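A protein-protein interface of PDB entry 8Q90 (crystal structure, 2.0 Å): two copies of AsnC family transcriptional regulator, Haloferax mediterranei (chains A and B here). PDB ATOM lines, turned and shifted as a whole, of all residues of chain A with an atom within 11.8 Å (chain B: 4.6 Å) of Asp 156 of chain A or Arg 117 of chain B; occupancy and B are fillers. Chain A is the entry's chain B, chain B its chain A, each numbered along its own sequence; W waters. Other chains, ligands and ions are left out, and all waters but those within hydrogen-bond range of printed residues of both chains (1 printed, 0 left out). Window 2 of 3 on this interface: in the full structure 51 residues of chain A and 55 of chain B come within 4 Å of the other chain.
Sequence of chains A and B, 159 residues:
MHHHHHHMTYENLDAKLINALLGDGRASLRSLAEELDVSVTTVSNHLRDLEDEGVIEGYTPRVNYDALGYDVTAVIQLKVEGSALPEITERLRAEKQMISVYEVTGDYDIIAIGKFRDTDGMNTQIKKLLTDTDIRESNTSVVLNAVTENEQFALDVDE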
ATOM      1  N   GLU A  11      12.113  12.614  17.191  1.00  0.00           N
ATOM      2  CA  GLU A  11      11.574  11.497  16.372  1.00  0.00           C
ATOM      3  C   GLU A  11      12.650  10.417  16.227  1.00  0.00           C
ATOM      4  O   GLU A  11      13.574  10.643  15.434  1.00  0.00           O
ATOM      5  CB  GLU A  11      11.093  12.009  15.017  1.00  0.00           C
ATOM      6  N   ASN A  12      12.531   9.319  16.976  1.00  0.00           N
ATOM      7  CA  ASN A  12      13.525   8.211  16.966  1.00  0.00           C
ATOM      8  C   ASN A  12      14.953   8.752  17.141  1.00  0.00           C
ATOM      9  O   ASN A  12      15.868   8.178  16.561  1.00  0.00           O
ATOM     10  CB  ASN A  12      13.329   7.280  15.764  1.00  0.00           C
ATOM     11  CG  ASN A  12      13.278   7.950  14.410  1.00  0.00           C
ATOM     12  OD1 ASN A  12      14.227   8.613  14.000  1.00  0.00           O
ATOM     13  ND2 ASN A  12      12.187   7.750  13.689  1.00  0.00           N
ATOM     14  N   LEU A  13      15.119   9.790  17.950  1.00  0.00           N
ATOM     15  CA  LEU A  13      16.450  10.413  18.130  1.00  0.00           C
ATOM     16  C   LEU A  13      17.353   9.478  18.938  1.00  0.00           C
ATOM     17  O   LEU A  13      18.473   9.246  18.505  1.00  0.00           O
ATOM     18  CB  LEU A  13      16.276  11.758  18.828  1.00  0.00           C
ATOM     19  CG  LEU A  13      17.535  12.619  18.875  1.00  0.00           C
ATOM     20  CD1 LEU A  13      18.098  12.826  17.479  1.00  0.00           C
ATOM     21  CD2 LEU A  13      17.259  13.953  19.551  1.00  0.00           C
ATOM     22  N   ASP A  14      16.844   8.949  20.045  1.00  0.00           N
ATOM     23  CA  ASP A  14      17.636   8.043  20.915  1.00  0.00           C
ATOM     24  C   ASP A  14      18.240   6.918  20.071  1.00  0.00           C
ATOM     25  O   ASP A  14      19.433   6.694  20.177  1.00  0.00           O
ATOM     26  CB  ASP A  14      16.784   7.521  22.072  1.00  0.00           C
ATOM     27  CG  ASP A  14      16.458   8.556  23.129  1.00  0.00           C
ATOM     28  OD1 ASP A  14      17.132   9.592  23.161  1.00  0.00           O
ATOM     29  OD2 ASP A  14      15.537   8.304  23.916  1.00  0.00           O
ATOM     30  N   ALA A  15      17.419   6.269  19.253  1.00  0.00           N
ATOM     31  CA  ALA A  15      17.892   5.169  18.385  1.00  0.00           C
ATOM     32  C   ALA A  15      18.989   5.668  17.446  1.00  0.00           C
ATOM     33  O   ALA A  15      19.982   4.966  17.261  1.00  0.00           O
ATOM     34  CB  ALA A  15      16.741   4.607  17.610  1.00  0.00           C
ATOM     35  N   LYS A  16      18.795   6.858  16.899  1.00  0.00           N
ATOM     36  CA  LYS A  16      19.765   7.407  15.920  1.00  0.00           C
ATOM     37  C   LYS A  16      21.029   7.804  16.683  1.00  0.00           C
ATOM     38  O   LYS A  16      22.111   7.635  16.147  1.00  0.00           O
ATOM     39  CB  LYS A  16      19.118   8.552  15.138  1.00  0.00           C
ATOM     40  CG  LYS A  16      18.077   8.110  14.122  1.00  0.00           C
ATOM     41  CD  LYS A  16      17.176   9.228  13.680  1.00  0.00           C
ATOM     42  CE  LYS A  16      17.905  10.545  13.555  1.00  0.00           C
ATOM     43  NZ  LYS A  16      17.072  11.553  12.862  1.00  0.00           N
ATOM     44  N   LEU A  17      20.860   8.292  17.901  1.00  0.00           N
ATOM     45  CA  LEU A  17      22.016   8.650  18.747  1.00  0.00           C
ATOM     46  C   LEU A  17      22.810   7.378  19.072  1.00  0.00           C
ATOM     47  O   LEU A  17      24.033   7.411  18.973  1.00  0.00           O
ATOM     48  CB  LEU A  17      21.509   9.351  20.008  1.00  0.00           C
ATOM     49  CG  LEU A  17      22.581   9.695  21.037  1.00  0.00           C
ATOM     50  CD1 LEU A  17      23.674  10.543  20.412  1.00  0.00           C
ATOM     51  CD2 LEU A  17      21.973  10.406  22.234  1.00  0.00           C
ATOM     52  N   ILE A  18      22.109   6.304  19.421  1.00  0.00           N
ATOM     53  CA  ILE A  18      22.796   5.033  19.783  1.00  0.00           C
ATOM     54  C   ILE A  18      23.521   4.537  18.533  1.00  0.00           C
ATOM     55  O   ILE A  18      24.702   4.225  18.627  1.00  0.00           O
ATOM     56  CB  ILE A  18      21.799   4.019  20.359  1.00  0.00           C
ATOM     57  CG1 ILE A  18      21.387   4.392  21.784  1.00  0.00           C
ATOM     58  CG2 ILE A  18      22.351   2.606  20.277  1.00  0.00           C
ATOM     59  CD1 ILE A  18      20.140   3.694  22.263  1.00  0.00           C
ATOM     60  N   ASN A  19      22.835   4.561  17.403  1.00  0.00           N
ATOM     61  CA  ASN A  19      23.423   4.104  16.121  1.00  0.00           C
ATOM     62  C   ASN A  19      24.614   4.990  15.739  1.00  0.00           C
ATOM     63  O   ASN A  19      25.577   4.460  15.196  1.00  0.00           O
ATOM     64  CB  ASN A  19      22.348   4.044  15.039  1.00  0.00           C
ATOM     65  CG  ASN A  19      21.331   2.954  15.292  1.00  0.00           C
ATOM     66  OD1 ASN A  19      21.481   2.170  16.220  1.00  0.00           O
ATOM     67  ND2 ASN A  19      20.296   2.899  14.474  1.00  0.00           N
ATOM     68  N   ALA A  20      24.623   6.260  16.098  1.00  0.00           N
ATOM     69  CA  ALA A  20      25.777   7.138  15.803  1.00  0.00           C
ATOM     70  C   ALA A  20      26.987   6.804  16.683  1.00  0.00           C
ATOM     71  O   ALA A  20      28.107   6.904  16.203  1.00  0.00           O
ATOM     72  CB  ALA A  20      25.354   8.568  15.975  1.00  0.00           C
ATOM     73  N   LEU A  22      27.633   3.853  18.043  1.00  0.00           N
ATOM     74  CA  LEU A  22      28.123   2.504  17.684  1.00  0.00           C
ATOM     75  C   LEU A  22      29.344   2.655  16.778  1.00  0.00           C
ATOM     76  O   LEU A  22      29.239   3.362  15.771  1.00  0.00           O
ATOM     77  CB  LEU A  22      26.988   1.740  17.004  1.00  0.00           C
ATOM     78  CG  LEU A  22      25.921   1.187  17.947  1.00  0.00           C
ATOM     79  CD1 LEU A  22      25.073   0.137  17.250  1.00  0.00           C
ATOM     80  CD2 LEU A  22      26.556   0.615  19.202  1.00  0.00           C
ATOM     81  N   LEU A  50      19.401   8.203  28.413  1.00  0.00           N
ATOM     82  CA  LEU A  50      19.666   6.786  28.033  1.00  0.00           C
ATOM     83  C   LEU A  50      20.565   6.082  29.065  1.00  0.00           C
ATOM     84  O   LEU A  50      20.362   4.900  29.301  1.00  0.00           O
ATOM     85  CB  LEU A  50      20.266   6.760  26.620  1.00  0.00           C
ATOM     86  CG  LEU A  50      19.303   7.140  25.499  1.00  0.00           C
ATOM     87  CD1 LEU A  50      20.055   7.460  24.219  1.00  0.00           C
ATOM     88  CD2 LEU A  50      18.287   6.035  25.260  1.00  0.00           C
ATOM     89  N   VAL A  55      19.826   2.098  29.333  1.00  0.00           N
ATOM     90  CA  VAL A  55      19.963   1.618  27.966  1.00  0.00           C
ATOM     91  C   VAL A  55      21.427   1.627  27.547  1.00  0.00           C
ATOM     92  O   VAL A  55      21.918   0.672  26.926  1.00  0.00           O
ATOM     93  CB  VAL A  55      19.083   2.460  27.030  1.00  0.00           C
ATOM     94  CG1 VAL A  55      19.292   2.029  25.601  1.00  0.00           C
ATOM     95  CG2 VAL A  55      17.612   2.317  27.439  1.00  0.00           C
ATOM     96  N   GLN A 152      27.682  -5.188  18.035  1.00  0.00           N
ATOM     97  CA  GLN A 152      26.338  -4.686  18.404  1.00  0.00           C
ATOM     98  C   GLN A 152      25.604  -4.206  17.149  1.00  0.00           C
ATOM     99  O   GLN A 152      26.204  -3.509  16.341  1.00  0.00           O
ATOM    100  CB  GLN A 152      26.487  -3.609  19.475  1.00  0.00           C
ATOM    101  CG  GLN A 152      27.095  -4.106  20.778  1.00  0.00           C
ATOM    102  CD  GLN A 152      27.261  -2.997  21.790  1.00  0.00           C
ATOM    103  OE1 GLN A 152      26.717  -3.047  22.888  1.00  0.00           O
ATOM    104  NE2 GLN A 152      28.022  -1.981  21.421  1.00  0.00           N
ATOM    105  N   PHE A 153      24.350  -4.602  17.018  1.00  0.00           N
ATOM    106  CA  PHE A 153      23.554  -4.237  15.826  1.00  0.00           C
ATOM    107  C   PHE A 153      22.920  -2.857  16.009  1.00  0.00           C
ATOM    108  O   PHE A 153      22.601  -2.459  17.124  1.00  0.00           O
ATOM    109  CB  PHE A 153      22.522  -5.322  15.506  1.00  0.00           C
ATOM    110  CG  PHE A 153      21.564  -5.702  16.603  1.00  0.00           C
ATOM    111  CD1 PHE A 153      20.355  -5.045  16.747  1.00  0.00           C
ATOM    112  CD2 PHE A 153      21.845  -6.756  17.457  1.00  0.00           C
ATOM    113  CE1 PHE A 153      19.462  -5.413  17.739  1.00  0.00           C
ATOM    114  CE2 PHE A 153      20.952  -7.120  18.450  1.00  0.00           C
ATOM    115  CZ  PHE A 153      19.762  -6.449  18.588  1.00  0.00           C
ATOM    116  N   ALA A 154      22.767  -2.156  14.899  1.00  0.00           N
ATOM    117  CA  ALA A 154      22.119  -0.838  14.934  1.00  0.00           C
ATOM    118  C   ALA A 154      20.625  -1.019  15.173  1.00  0.00           C
ATOM    119  O   ALA A 154      20.069  -2.044  14.755  1.00  0.00           O
ATOM    120  CB  ALA A 154      22.378  -0.098  13.658  1.00  0.00           C
ATOM    121  N   LEU A 155      20.026  -0.039  15.823  1.00  0.00           N
ATOM    122  CA  LEU A 155      18.596  -0.097  16.169  1.00  0.00           C
ATOM    123  C   LEU A 155      17.747   0.308  14.962  1.00  0.00           C
ATOM    124  O   LEU A 155      18.212   1.119  14.166  1.00  0.00           O
ATOM    125  CB  LEU A 155      18.375   0.816  17.376  1.00  0.00           C
ATOM    126  CG  LEU A 155      19.197   0.478  18.617  1.00  0.00           C
ATOM    127  CD1 LEU A 155      18.767   1.335  19.794  1.00  0.00           C
ATOM    128  CD2 LEU A 155      19.074  -0.996  18.962  1.00  0.00           C
ATOM    129  N   ASP A 156      16.561  -0.268  14.852  1.00  0.00           N
ATOM    130  CA  ASP A 156      15.617   0.055  13.763  1.00  0.00           C
ATOM    131  C   ASP A 156      15.186   1.513  13.885  1.00  0.00           C
ATOM    132  O   ASP A 156      14.826   1.921  14.992  1.00  0.00           O
ATOM    133  CB  ASP A 156      14.428  -0.901  13.808  1.00  0.00           C
ATOM    134  CG  ASP A 156      14.643  -2.178  13.017  1.00  0.00           C
ATOM    135  OD1 ASP A 156      15.682  -2.281  12.338  1.00  0.00           O
ATOM    136  OD2 ASP A 156      13.765  -3.060  13.089  1.00  0.00           O
ATOM    137  N   VAL A 157      15.290   2.275  12.801  1.00  0.00           N
ATOM    138  CA  VAL A 157      14.797   3.683  12.792  1.00  0.00           C
ATOM    139  C   VAL A 157      13.788   3.825  11.644  1.00  0.00           C
ATOM    140  O   VAL A 157      12.831   4.604  11.813  1.00  0.00           O
ATOM    141  CB  VAL A 157      15.948   4.696  12.652  1.00  0.00           C
ATOM    142  CG1 VAL A 157      15.449   6.125  12.524  1.00  0.00           C
ATOM    143  CG2 VAL A 157      16.951   4.578  13.790  1.00  0.00           C
ATOM    144  N   LEU B  68      15.942  -2.834  25.361  1.00  0.00           N
ATOM    145  CA  LEU B  68      15.368  -2.484  24.040  1.00  0.00           C
ATOM    146  C   LEU B  68      14.447  -3.600  23.532  1.00  0.00           C
ATOM    147  O   LEU B  68      14.113  -3.565  22.350  1.00  0.00           O
ATOM    148  CB  LEU B  68      16.531  -2.265  23.074  1.00  0.00           C
ATOM    149  CG  LEU B  68      17.535  -1.191  23.487  1.00  0.00           C
ATOM    150  CD1 LEU B  68      18.697  -1.141  22.516  1.00  0.00           C
ATOM    151  CD2 LEU B  68      16.868   0.170  23.586  1.00  0.00           C
ATOM    152  N   GLY B  69      14.082  -4.555  24.383  1.00  0.00           N
ATOM    153  CA  GLY B  69      13.132  -5.613  23.993  1.00  0.00           C
ATOM    154  C   GLY B  69      13.777  -6.825  23.352  1.00  0.00           C
ATOM    155  O   GLY B  69      13.049  -7.650  22.808  1.00  0.00           O
ATOM    156  N   TYR B  70      15.098  -6.922  23.411  1.00  0.00           N
ATOM    157  CA  TYR B  70      15.757  -8.115  22.894  1.00  0.00           C
ATOM    158  C   TYR B  70      16.057  -9.012  24.094  1.00  0.00           C
ATOM    159  O   TYR B  70      17.169  -9.070  24.604  1.00  0.00           O
ATOM    160  CB  TYR B  70      16.998  -7.742  22.083  1.00  0.00           C
ATOM    161  CG  TYR B  70      16.660  -7.155  20.725  1.00  0.00           C
ATOM    162  CD1 TYR B  70      16.379  -7.975  19.658  1.00  0.00           C
ATOM    163  CD2 TYR B  70      16.620  -5.783  20.516  1.00  0.00           C
ATOM    164  CE1 TYR B  70      16.068  -7.461  18.422  1.00  0.00           C
ATOM    165  CE2 TYR B  70      16.305  -5.254  19.273  1.00  0.00           C
ATOM    166  CZ  TYR B  70      16.034  -6.107  18.233  1.00  0.00           C
ATOM    167  OH  TYR B  70      15.723  -5.630  16.978  1.00  0.00           O
ATOM    168  N   ASP B  71      15.021  -9.735  24.539  1.00  0.00           N
ATOM    169  CA  ASP B  71      15.083 -10.470  25.793  1.00  0.00           C
ATOM    170  C   ASP B  71      15.826 -11.795  25.701  1.00  0.00           C
ATOM    171  O   ASP B  71      16.246 -12.314  26.741  1.00  0.00           O
ATOM    172  CB  ASP B  71      13.678 -10.784  26.322  1.00  0.00           C
ATOM    173  CG  ASP B  71      12.812  -9.540  26.512  1.00  0.00           C
ATOM    174  OD1 ASP B  71      13.347  -8.405  26.477  1.00  0.00           O
ATOM    175  OD2 ASP B  71      11.579  -9.714  26.710  1.00  0.00           O
ATOM    176  N   VAL B  72      15.948 -12.386  24.516  1.00  0.00           N
ATOM    177  CA  VAL B  72      16.403 -13.768  24.383  1.00  0.00           C
ATOM    178  C   VAL B  72      17.756 -13.799  23.697  1.00  0.00           C
ATOM    179  O   VAL B  72      17.968 -13.109  22.699  1.00  0.00           O
ATOM    180  CB  VAL B  72      15.379 -14.619  23.607  1.00  0.00           C
ATOM    181  CG1 VAL B  72      15.993 -15.941  23.182  1.00  0.00           C
ATOM    182  CG2 VAL B  72      14.166 -14.870  24.480  1.00  0.00           C
ATOM    183  N   LYS B  96      22.058  -9.019  11.346  1.00  0.00           N
ATOM    184  CA  LYS B  96      22.660  -8.124  12.362  1.00  0.00           C
ATOM    185  C   LYS B  96      22.448  -8.663  13.779  1.00  0.00           C
ATOM    186  O   LYS B  96      23.243  -8.308  14.646  1.00  0.00           O
ATOM    187  CB  LYS B  96      22.056  -6.727  12.221  1.00  0.00           C
ATOM    188  CG  LYS B  96      20.647  -6.572  12.772  1.00  0.00           C
ATOM    189  CD  LYS B  96      20.054  -5.211  12.506  1.00  0.00           C
ATOM    190  CE  LYS B  96      18.650  -5.069  13.047  1.00  0.00           C
ATOM    191  NZ  LYS B  96      18.161  -3.675  12.935  1.00  0.00           N
ATOM    192  N   PHE B 116      17.443 -11.900  20.300  1.00  0.00           N
ATOM    193  CA  PHE B 116      16.122 -11.985  19.689  1.00  0.00           C
ATOM    194  C   PHE B 116      15.085 -11.325  20.585  1.00  0.00           C
ATOM    195  O   PHE B 116      15.261 -11.246  21.798  1.00  0.00           O
ATOM    196  CB  PHE B 116      15.726 -13.449  19.421  1.00  0.00           C
ATOM    197  CG  PHE B 116      16.728 -14.203  18.591  1.00  0.00           C
ATOM    198  CD1 PHE B 116      16.671 -14.152  17.206  1.00  0.00           C
ATOM    199  CD2 PHE B 116      17.733 -14.946  19.193  1.00  0.00           C
ATOM    200  CE1 PHE B 116      17.594 -14.834  16.445  1.00  0.00           C
ATOM    201  CE2 PHE B 116      18.672 -15.629  18.434  1.00  0.00           C
ATOM    202  CZ  PHE B 116      18.598 -15.577  17.060  1.00  0.00           C
ATOM    203  N   ARG B 117      13.979 -10.871  19.972  1.00  0.00           N
ATOM    204  CA  ARG B 117      12.944 -10.186  20.747  1.00  0.00           C
ATOM    205  C   ARG B 117      12.322 -11.117  21.774  1.00  0.00           C
ATOM    206  O   ARG B 117      12.020 -10.700  22.897  1.00  0.00           O
ATOM    207  CB  ARG B 117      11.856  -9.615  19.836  1.00  0.00           C
ATOM    208  CG  ARG B 117      12.368  -8.717  18.711  1.00  0.00           C
ATOM    209  CD  ARG B 117      11.874  -7.296  18.885  1.00  0.00           C
ATOM    210  NE  ARG B 117      12.109  -6.504  17.684  1.00  0.00           N
ATOM    211  CZ  ARG B 117      12.428  -5.213  17.693  1.00  0.00           C
ATOM    212  NH1 ARG B 117      12.559  -4.565  18.853  1.00  0.00           N
ATOM    213  NH2 ARG B 117      12.629  -4.573  16.542  1.00  0.00           N
ATOM    214  N   ASP B 118      12.129 -12.376  21.411  1.00  0.00           N
ATOM    215  CA  ASP B 118      11.495 -13.365  22.272  1.00  0.00           C
ATOM    216  C   ASP B 118      11.717 -14.731  21.637  1.00  0.00           C
ATOM    217  O   ASP B 118      12.345 -14.854  20.580  1.00  0.00           O
ATOM    218  CB  ASP B 118      10.004 -13.061  22.470  1.00  0.00           C
ATOM    219  CG  ASP B 118       9.243 -12.934  21.155  1.00  0.00           C
ATOM    220  OD1 ASP B 118       9.584 -13.615  20.163  1.00  0.00           O
ATOM    221  OD2 ASP B 118       8.294 -12.130  21.103  1.00  0.00           O
HETATM  222  O   HOH W   1      15.989  -2.339  17.125  1.00  0.00           O
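Leu 68 of chain B touches Val 55 of chain A.
Tyr 70 of chain B touches Phe 153 of chain A (CE2 to CE1, 3.5 Å).
O of Lys 96 of chain B touches CB of Phe 153 of chain A, 3.2 Å away.
Leu 68 of chain B touches Leu 155 of chain A (CD1 to CD2, 3.6 Å).
The backbone NH of Leu 155 of chain A lies within hydrogen-bond range of the side-chain amide oxygen of Asn 19 of chain A (2.7 Å).
The side-chain hydroxyl (OH) of Tyr 70 of chain B is in hydrogen-bond range of the guanidinium group (NH2) of Arg 117 of chain B (3.3 Å).
The backbone carbonyl oxygen (O) of Leu 50 of chain A is in hydrogen-bond range of the backbone NH (N) of Val 55 of chain A.
Lys 16 of chain A touches none of the printed residues of chain B.
Printed residues of chain B within 4 Å of Phe 153 of chain A: Tyr 70 and Lys 96.
Printed residues of chain B within 4 Å of Ala 154 of chain A: Lys 96 (3.1 Å).
Of the printed residues of chain B, Asp 156 of chain A touches Lys 96 (2.9 Å) and Arg 117 (3.9 Å).
Val 157 of chain A touches none of the printed residues of chain B.
Of the printed residues of chain A, Leu 68 of chain B touches Val 55 (3.7 Å) and Leu 155 (3.6 Å).
No residue of chain A comes within 4 Å of Gly 69 of chain B.
No residue of chain A comes within 4 Å of Val 72 of chain B.
Phe 116 of chain B touches none of the printed residues of chain A.
Of chain A, only Asp 156 comes within 4 Å of Arg 117 of chain B.
The nearest printed residue of chain B that does not touch Asp 156 of chain A is Tyr 70 of chain B (5.1 Å).
The nearest printed residue of chain B that does not touch Phe 153 of chain A is Phe 116 of chain B (6.2 Å).
The side-chain amino group (NZ) of Lys 96 of chain B lies within hydrogen-bond range of the backbone carbonyl oxygen (O) of Ala 154 of chain A (3.1 Å).
The side-chain carboxylate (OD2) of Asp 156 of chain A lies within salt-bridge range of the guanidinium group (NH2) of Arg 117 of chain B (3.9 Å).
NZ of Lys 96 of chain B lies within salt-bridge range of OD1 of Asp 156 of chain A (2.9 Å).
No position is printed for both chains.
Water W1 bridges the backbone NH of Asp 156 of chain A (3.1 Å) and the side-chain hydroxyl of Tyr 70 of chain B (3.3 Å).
Printed residues of chain B that touch a printed residue of chain A: Leu 68, Tyr 70, Lys 96 and Arg 117.
Hydrophobic or aromatic side chains of chain B that line the printed part of chain A: Leu 68 and Tyr 70.
Printed residues of chain A that touch a printed residue of chain B: Val 55, Phe 153, Ala 154, Leu 155 and Asp 156.
Along chain A the printed residues that touch a printed residue of chain B span positions 55 to 156.
Among the printed residues, 7 pairs touch across the chains.
Among the printed residues, Asp or Glu carboxylates within 4 Å of a Lys or Arg side-chain nitrogen of the other chain: Asp 156 of chain A with Lys 96 of chain B and Asp 156 of chain A with Arg 117 of chain B.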
